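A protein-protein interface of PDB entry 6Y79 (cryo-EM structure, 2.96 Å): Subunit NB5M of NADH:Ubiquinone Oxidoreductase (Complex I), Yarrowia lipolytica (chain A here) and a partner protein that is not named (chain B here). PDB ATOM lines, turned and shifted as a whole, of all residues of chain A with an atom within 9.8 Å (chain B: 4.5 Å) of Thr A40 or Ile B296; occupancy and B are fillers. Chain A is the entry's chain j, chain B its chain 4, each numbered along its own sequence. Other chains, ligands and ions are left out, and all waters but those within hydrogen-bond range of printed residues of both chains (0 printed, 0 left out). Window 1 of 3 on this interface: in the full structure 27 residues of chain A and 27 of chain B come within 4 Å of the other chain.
The backbone NH (N) of Val B359 lies within hydrogen-bond range of the backbone carbonyl oxygen (O) of Ile B296 (2.8 Å). The backbone carbonyl oxygen (O) of Ala A36 is in hydrogen-bond range of the side-chain hydroxyl (OG1) of Thr A40 (2.8 Å). The side-chain hydroxyl of Tyr A35 lies within hydrogen-bond range of the guanidinium group of Arg A39, at 2.5 Å. O of Thr A40 sits close to OE1 of Gln A43, 3.4 Å away.
Among the printed residues, merely in contact across the chains: Ile A32 with Ile B358, Asp A33 with Ile B358, Tyr A35 with Ile B296, Ala A36 with Ile B296, Ala A36 with Ile B358, Arg A39 with Arg B294, Arg A39 with Ile B296 and Thr A40 with Ile B296.
Hydrophobic or aromatic side chains of chain A within 4 Å of the printed part of chain B: Ile A32, Tyr A35 and Ala A36. Among the printed residues, 8 pairs touch across the chains.
Thr A40 touches just one residue of chain B: Ile B296 (3.8 Å). Of the printed residues of chain B, Ala A36 touches Ile B296 and Ile B358. Printed residues of chain B within 4 Å of Arg A39: Arg B294 (3.8 Å) and Ile B296 (3.7 Å). Printed residues of chain B within 4 Å of Asp A33: Ile B358. Of the printed residues of chain B, Tyr A35 touches Ile B296. Printed residues of chain A within 4 Å of Ile B358: Ile A32, Asp A33 and Ala A36. Gln A43 touches none of the printed residues of chain B. Tyr A42 touches none of the printed residues of chain B. The nearest printed residue of chain B that does not touch Tyr A35 is Arg B294 (5.6 Å).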
ATOM      1  N   ALA A  31      25.741 -25.787  12.575  1.00  0.00           N
ATOM      2  CA  ALA A  31      24.414 -25.797  11.965  1.00  0.00           C
ATOM      3  C   ALA A  31      23.614 -24.558  12.342  1.00  0.00           C
ATOM      4  O   ALA A  31      22.950 -23.968  11.484  1.00  0.00           O
ATOM      5  CB  ALA A  31      23.655 -27.060  12.363  1.00  0.00           C
ATOM      6  N   ILE A  32      23.675 -24.137  13.608  1.00  0.00           N
ATOM      7  CA  ILE A  32      22.953 -22.940  14.029  1.00  0.00           C
ATOM      8  C   ILE A  32      23.574 -21.695  13.409  1.00  0.00           C
ATOM      9  O   ILE A  32      22.860 -20.776  12.994  1.00  0.00           O
ATOM     10  CB  ILE A  32      22.901 -22.858  15.567  1.00  0.00           C
ATOM     11  CG1 ILE A  32      22.182 -24.074  16.141  1.00  0.00           C
ATOM     12  CG2 ILE A  32      22.175 -21.611  16.038  1.00  0.00           C
ATOM     13  CD1 ILE A  32      22.155 -24.098  17.641  1.00  0.00           C
ATOM     14  N   ASP A  33      24.907 -21.663  13.293  1.00  0.00           N
ATOM     15  CA  ASP A  33      25.570 -20.522  12.666  1.00  0.00           C
ATOM     16  C   ASP A  33      25.247 -20.438  11.183  1.00  0.00           C
ATOM     17  O   ASP A  33      25.012 -19.345  10.662  1.00  0.00           O
ATOM     18  CB  ASP A  33      27.082 -20.592  12.873  1.00  0.00           C
ATOM     19  CG  ASP A  33      27.492 -20.306  14.301  1.00  0.00           C
ATOM     20  OD1 ASP A  33      26.691 -19.701  15.040  1.00  0.00           O
ATOM     21  OD2 ASP A  33      28.611 -20.698  14.692  1.00  0.00           O
ATOM     22  N   ARG A  34      25.195 -21.580  10.494  1.00  0.00           N
ATOM     23  CA  ARG A  34      24.850 -21.570   9.075  1.00  0.00           C
ATOM     24  C   ARG A  34      23.386 -21.211   8.859  1.00  0.00           C
ATOM     25  O   ARG A  34      23.056 -20.474   7.925  1.00  0.00           O
ATOM     26  CB  ARG A  34      25.165 -22.925   8.447  1.00  0.00           C
ATOM     27  CG  ARG A  34      26.641 -23.136   8.161  1.00  0.00           C
ATOM     28  CD  ARG A  34      26.894 -24.436   7.416  1.00  0.00           C
ATOM     29  NE  ARG A  34      26.315 -25.592   8.094  1.00  0.00           N
ATOM     30  CZ  ARG A  34      26.981 -26.386   8.926  1.00  0.00           C
ATOM     31  NH1 ARG A  34      26.366 -27.415   9.494  1.00  0.00           N
ATOM     32  NH2 ARG A  34      28.259 -26.154   9.194  1.00  0.00           N
ATOM     33  N   TYR A  35      22.505 -21.692   9.736  1.00  0.00           N
ATOM     34  CA  TYR A  35      21.087 -21.349   9.676  1.00  0.00           C
ATOM     35  C   TYR A  35      20.862 -19.861   9.899  1.00  0.00           C
ATOM     36  O   TYR A  35      20.096 -19.216   9.174  1.00  0.00           O
ATOM     37  CB  TYR A  35      20.341 -22.165  10.726  1.00  0.00           C
ATOM     38  CG  TYR A  35      18.902 -21.801  10.902  1.00  0.00           C
ATOM     39  CD1 TYR A  35      17.986 -22.070   9.911  1.00  0.00           C
ATOM     40  CD2 TYR A  35      18.450 -21.217  12.075  1.00  0.00           C
ATOM     41  CE1 TYR A  35      16.666 -21.749  10.065  1.00  0.00           C
ATOM     42  CE2 TYR A  35      17.121 -20.897  12.242  1.00  0.00           C
ATOM     43  CZ  TYR A  35      16.237 -21.168  11.232  1.00  0.00           C
ATOM     44  OH  TYR A  35      14.912 -20.851  11.384  1.00  0.00           O
ATOM     45  N   ALA A  36      21.546 -19.293  10.886  1.00  0.00           N
ATOM     46  CA  ALA A  36      21.333 -17.896  11.212  1.00  0.00           C
ATOM     47  C   ALA A  36      21.985 -16.970  10.206  1.00  0.00           C
ATOM     48  O   ALA A  36      21.431 -15.909   9.907  1.00  0.00           O
ATOM     49  CB  ALA A  36      21.862 -17.611  12.601  1.00  0.00           C
ATOM     50  N   HIS A  37      23.151 -17.346   9.678  1.00  0.00           N
ATOM     51  CA  HIS A  37      23.734 -16.598   8.576  1.00  0.00           C
ATOM     52  C   HIS A  37      22.871 -16.687   7.332  1.00  0.00           C
ATOM     53  O   HIS A  37      22.867 -15.766   6.513  1.00  0.00           O
ATOM     54  CB  HIS A  37      25.136 -17.109   8.272  1.00  0.00           C
ATOM     55  CG  HIS A  37      25.875 -16.275   7.277  1.00  0.00           C
ATOM     56  ND1 HIS A  37      25.684 -16.397   5.918  1.00  0.00           N
ATOM     57  CD2 HIS A  37      26.803 -15.305   7.442  1.00  0.00           C
ATOM     58  CE1 HIS A  37      26.464 -15.538   5.289  1.00  0.00           C
ATOM     59  NE2 HIS A  37      27.154 -14.865   6.190  1.00  0.00           N
ATOM     60  N   TRP A  38      22.138 -17.783   7.175  1.00  0.00           N
ATOM     61  CA  TRP A  38      21.222 -17.891   6.057  1.00  0.00           C
ATOM     62  C   TRP A  38      20.002 -17.000   6.234  1.00  0.00           C
ATOM     63  O   TRP A  38      19.484 -16.469   5.246  1.00  0.00           O
ATOM     64  CB  TRP A  38      20.802 -19.347   5.889  1.00  0.00           C
ATOM     65  CG  TRP A  38      19.983 -19.559   4.693  1.00  0.00           C
ATOM     66  CD1 TRP A  38      20.430 -19.837   3.446  1.00  0.00           C
ATOM     67  CD2 TRP A  38      18.563 -19.495   4.607  1.00  0.00           C
ATOM     68  NE1 TRP A  38      19.377 -19.954   2.585  1.00  0.00           N
ATOM     69  CE2 TRP A  38      18.216 -19.743   3.275  1.00  0.00           C
ATOM     70  CE3 TRP A  38      17.549 -19.246   5.529  1.00  0.00           C
ATOM     71  CZ2 TRP A  38      16.903 -19.755   2.841  1.00  0.00           C
ATOM     72  CZ3 TRP A  38      16.251 -19.254   5.095  1.00  0.00           C
ATOM     73  CH2 TRP A  38      15.937 -19.506   3.764  1.00  0.00           C
ATOM     74  N   ARG A  39      19.513 -16.855   7.471  1.00  0.00           N
ATOM     75  CA  ARG A  39      18.311 -16.057   7.708  1.00  0.00           C
ATOM     76  C   ARG A  39      18.602 -14.561   7.718  1.00  0.00           C
ATOM     77  O   ARG A  39      17.762 -13.767   7.284  1.00  0.00           O
ATOM     78  CB  ARG A  39      17.670 -16.449   9.031  1.00  0.00           C
ATOM     79  CG  ARG A  39      17.104 -17.843   9.112  1.00  0.00           C
ATOM     80  CD  ARG A  39      15.781 -17.944   8.403  1.00  0.00           C
ATOM     81  NE  ARG A  39      14.774 -17.113   9.047  1.00  0.00           N
ATOM     82  CZ  ARG A  39      13.962 -17.520  10.013  1.00  0.00           C
ATOM     83  NH1 ARG A  39      13.086 -16.680  10.537  1.00  0.00           N
ATOM     84  NH2 ARG A  39      14.021 -18.761  10.462  1.00  0.00           N
ATOM     85  N   THR A  40      19.756 -14.166   8.271  1.00  0.00           N
ATOM     86  CA  THR A  40      20.141 -12.759   8.344  1.00  0.00           C
ATOM     87  C   THR A  40      20.280 -12.139   6.962  1.00  0.00           C
ATOM     88  O   THR A  40      19.839 -11.006   6.740  1.00  0.00           O
ATOM     89  CB  THR A  40      21.455 -12.622   9.116  1.00  0.00           C
ATOM     90  OG1 THR A  40      21.306 -13.184  10.423  1.00  0.00           O
ATOM     91  CG2 THR A  40      21.877 -11.165   9.259  1.00  0.00           C
ATOM     92  N   PHE A  41      20.846 -12.873   6.013  1.00  0.00           N
ATOM     93  CA  PHE A  41      21.091 -12.369   4.671  1.00  0.00           C
ATOM     94  C   PHE A  41      20.101 -12.947   3.671  1.00  0.00           C
ATOM     95  O   PHE A  41      20.463 -13.258   2.538  1.00  0.00           O
ATOM     96  CB  PHE A  41      22.529 -12.664   4.262  1.00  0.00           C
ATOM     97  CG  PHE A  41      23.550 -11.968   5.120  1.00  0.00           C
ATOM     98  CD1 PHE A  41      23.270 -10.739   5.697  1.00  0.00           C
ATOM     99  CD2 PHE A  41      24.774 -12.551   5.373  1.00  0.00           C
ATOM    100  CE1 PHE A  41      24.191 -10.108   6.494  1.00  0.00           C
ATOM    101  CE2 PHE A  41      25.704 -11.916   6.172  1.00  0.00           C
ATOM    102  CZ  PHE A  41      25.408 -10.695   6.731  1.00  0.00           C
ATOM    103  N   TYR A  42      18.838 -13.070   4.091  1.00  0.00           N
ATOM    104  CA  TYR A  42      17.809 -13.750   3.309  1.00  0.00           C
ATOM    105  C   TYR A  42      17.443 -12.978   2.054  1.00  0.00           C
ATOM    106  O   TYR A  42      16.949 -13.558   1.086  1.00  0.00           O
ATOM    107  CB  TYR A  42      16.570 -13.952   4.179  1.00  0.00           C
ATOM    108  CG  TYR A  42      15.390 -14.600   3.498  1.00  0.00           C
ATOM    109  CD1 TYR A  42      15.334 -15.968   3.334  1.00  0.00           C
ATOM    110  CD2 TYR A  42      14.330 -13.837   3.026  1.00  0.00           C
ATOM    111  CE1 TYR A  42      14.261 -16.562   2.715  1.00  0.00           C
ATOM    112  CE2 TYR A  42      13.258 -14.420   2.402  1.00  0.00           C
ATOM    113  CZ  TYR A  42      13.227 -15.782   2.252  1.00  0.00           C
ATOM    114  OH  TYR A  42      12.153 -16.371   1.636  1.00  0.00           O
ATOM    115  N   GLN A  43      17.684 -11.679   2.054  1.00  0.00           N
ATOM    116  CA  GLN A  43      17.189 -10.800   1.012  1.00  0.00           C
ATOM    117  C   GLN A  43      17.995 -10.869  -0.273  1.00  0.00           C
ATOM    118  O   GLN A  43      17.470 -10.521  -1.333  1.00  0.00           O
ATOM    119  CB  GLN A  43      17.204  -9.383   1.532  1.00  0.00           C
ATOM    120  CG  GLN A  43      18.595  -8.883   1.892  1.00  0.00           C
ATOM    121  CD  GLN A  43      18.938  -9.076   3.336  1.00  0.00           C
ATOM    122  OE1 GLN A  43      18.211  -9.727   4.073  1.00  0.00           O
ATOM    123  NE2 GLN A  43      20.060  -8.514   3.755  1.00  0.00           N
ATOM    124  N   GLU A  44      19.259 -11.275  -0.207  1.00  0.00           N
ATOM    125  CA  GLU A  44      20.075 -11.320  -1.400  1.00  0.00           C
ATOM    126  C   GLU A  44      19.850 -12.598  -2.183  1.00  0.00           C
ATOM    127  O   GLU A  44      20.355 -12.727  -3.302  1.00  0.00           O
ATOM    128  CB  GLU A  44      21.552 -11.173  -1.031  1.00  0.00           C
ATOM    129  CG  GLU A  44      21.945  -9.814  -0.441  1.00  0.00           C
ATOM    130  CD  GLU A  44      21.839  -8.655  -1.435  1.00  0.00           C
ATOM    131  OE1 GLU A  44      21.943  -8.895  -2.656  1.00  0.00           O
ATOM    132  OE2 GLU A  44      21.680  -7.495  -0.993  1.00  0.00           O
ATOM    133  N   ARG A  45      19.102 -13.539  -1.615  1.00  0.00           N
ATOM    134  CA  ARG A  45      18.660 -14.733  -2.313  1.00  0.00           C
ATOM    135  C   ARG A  45      17.149 -14.752  -2.466  1.00  0.00           C
ATOM    136  O   ARG A  45      16.593 -15.761  -2.903  1.00  0.00           O
ATOM    137  CB  ARG A  45      19.144 -15.985  -1.580  1.00  0.00           C
ATOM    138  CG  ARG A  45      18.588 -16.121  -0.183  1.00  0.00           C
ATOM    139  CD  ARG A  45      19.140 -17.336   0.509  1.00  0.00           C
ATOM    140  NE  ARG A  45      20.563 -17.215   0.785  1.00  0.00           N
ATOM    141  CZ  ARG A  45      21.054 -16.689   1.899  1.00  0.00           C
ATOM    142  NH1 ARG A  45      20.225 -16.246   2.831  1.00  0.00           N
ATOM    143  NH2 ARG A  45      22.365 -16.610   2.089  1.00  0.00           N
ATOM    144  N   ARG B 294       8.861 -14.092  14.051  1.00  0.00           N
ATOM    145  CA  ARG B 294       9.804 -14.962  13.372  1.00  0.00           C
ATOM    146  C   ARG B 294      11.126 -14.215  13.253  1.00  0.00           C
ATOM    147  O   ARG B 294      11.449 -13.643  12.216  1.00  0.00           O
ATOM    148  CB  ARG B 294       9.248 -15.352  12.044  1.00  0.00           C
ATOM    149  CG  ARG B 294       7.875 -15.993  12.143  1.00  0.00           C
ATOM    150  CD  ARG B 294       7.984 -17.425  12.606  1.00  0.00           C
ATOM    151  NE  ARG B 294       8.977 -18.134  11.816  1.00  0.00           N
ATOM    152  CZ  ARG B 294       8.719 -18.744  10.670  1.00  0.00           C
ATOM    153  NH1 ARG B 294       7.491 -18.745  10.181  1.00  0.00           N
ATOM    154  NH2 ARG B 294       9.690 -19.354  10.018  1.00  0.00           N
ATOM    155  N   GLN B 295      11.906 -14.247  14.328  1.00  0.00           N
ATOM    156  CA  GLN B 295      13.213 -13.605  14.369  1.00  0.00           C
ATOM    157  C   GLN B 295      14.186 -14.549  15.050  1.00  0.00           C
ATOM    158  O   GLN B 295      13.903 -15.070  16.130  1.00  0.00           O
ATOM    159  CB  GLN B 295      13.187 -12.268  15.120  1.00  0.00           C
ATOM    160  CG  GLN B 295      12.387 -11.157  14.466  1.00  0.00           C
ATOM    161  CD  GLN B 295      12.942 -10.728  13.134  1.00  0.00           C
ATOM    162  OE1 GLN B 295      14.148 -10.634  12.957  1.00  0.00           O
ATOM    163  NE2 GLN B 295      12.060 -10.456  12.188  1.00  0.00           N
ATOM    164  N   ILE B 296      15.327 -14.764  14.407  1.00  0.00           N
ATOM    165  CA  ILE B 296      16.348 -15.655  14.932  1.00  0.00           C
ATOM    166  C   ILE B 296      17.354 -14.941  15.821  1.00  0.00           C
ATOM    167  O   ILE B 296      18.105 -15.601  16.548  1.00  0.00           O
ATOM    168  CB  ILE B 296      17.108 -16.300  13.770  1.00  0.00           C
ATOM    169  CG1 ILE B 296      17.625 -15.169  12.906  1.00  0.00           C
ATOM    170  CG2 ILE B 296      16.173 -17.132  12.940  1.00  0.00           C
ATOM    171  CD1 ILE B 296      18.911 -15.404  12.319  1.00  0.00           C
ATOM    172  N   ASP B 297      17.421 -13.623  15.748  1.00  0.00           N
ATOM    173  CA  ASP B 297      18.436 -12.822  16.399  1.00  0.00           C
ATOM    174  C   ASP B 297      17.772 -12.086  17.548  1.00  0.00           C
ATOM    175  O   ASP B 297      16.551 -12.029  17.650  1.00  0.00           O
ATOM    176  CB  ASP B 297      19.079 -11.888  15.364  1.00  0.00           C
ATOM    177  CG  ASP B 297      20.316 -11.162  15.865  1.00  0.00           C
ATOM    178  OD1 ASP B 297      20.606 -11.199  17.072  1.00  0.00           O
ATOM    179  OD2 ASP B 297      20.997 -10.512  15.043  1.00  0.00           O
ATOM    180  N   LEU B 298      18.587 -11.543  18.428  1.00  0.00           N
ATOM    181  CA  LEU B 298      18.128 -11.165  19.749  1.00  0.00           C
ATOM    182  C   LEU B 298      18.032  -9.672  19.959  1.00  0.00           C
ATOM    183  O   LEU B 298      17.155  -9.221  20.695  1.00  0.00           O
ATOM    184  CB  LEU B 298      19.074 -11.759  20.784  1.00  0.00           C
ATOM    185  CG  LEU B 298      18.666 -11.945  22.222  1.00  0.00           C
ATOM    186  CD1 LEU B 298      17.284 -12.457  22.304  1.00  0.00           C
ATOM    187  CD2 LEU B 298      19.574 -12.990  22.680  1.00  0.00           C
ATOM    188  N   ARG B 357      24.601 -13.799  19.124  1.00  0.00           N
ATOM    189  CA  ARG B 357      23.317 -13.165  19.381  1.00  0.00           C
ATOM    190  C   ARG B 357      22.147 -13.983  18.865  1.00  0.00           C
ATOM    191  O   ARG B 357      21.025 -13.481  18.827  1.00  0.00           O
ATOM    192  CB  ARG B 357      23.290 -11.771  18.761  1.00  0.00           C
ATOM    193  CG  ARG B 357      24.049 -10.712  19.522  1.00  0.00           C
ATOM    194  CD  ARG B 357      23.965  -9.387  18.796  1.00  0.00           C
ATOM    195  NE  ARG B 357      24.799  -8.364  19.416  1.00  0.00           N
ATOM    196  CZ  ARG B 357      25.149  -7.231  18.819  1.00  0.00           C
ATOM    197  NH1 ARG B 357      24.739  -6.982  17.587  1.00  0.00           N
ATOM    198  NH2 ARG B 357      25.909  -6.350  19.450  1.00  0.00           N
ATOM    199  N   ILE B 358      22.380 -15.228  18.463  1.00  0.00           N
ATOM    200  CA  ILE B 358      21.309 -16.064  17.948  1.00  0.00           C
ATOM    201  C   ILE B 358      20.486 -16.596  19.114  1.00  0.00           C
ATOM    202  O   ILE B 358      21.016 -16.863  20.198  1.00  0.00           O
ATOM    203  CB  ILE B 358      21.914 -17.183  17.086  1.00  0.00           C
ATOM    204  CG1 ILE B 358      22.905 -16.574  16.098  1.00  0.00           C
ATOM    205  CG2 ILE B 358      20.855 -17.927  16.314  1.00  0.00           C
ATOM    206  CD1 ILE B 358      23.922 -17.544  15.554  1.00  0.00           C
ATOM    207  N   VAL B 359      19.170 -16.711  18.905  1.00  0.00           N
ATOM    208  CA  VAL B 359      18.244 -17.093  19.969  1.00  0.00           C
ATOM    209  C   VAL B 359      18.396 -18.567  20.330  1.00  0.00           C
ATOM    210  O   VAL B 359      18.098 -18.970  21.462  1.00  0.00           O
ATOM    211  CB  VAL B 359      16.797 -16.742  19.550  1.00  0.00           C
ATOM    212  CG1 VAL B 359      16.308 -17.618  18.406  1.00  0.00           C
ATOM    213  CG2 VAL B 359      15.832 -16.817  20.717  1.00  0.00           C
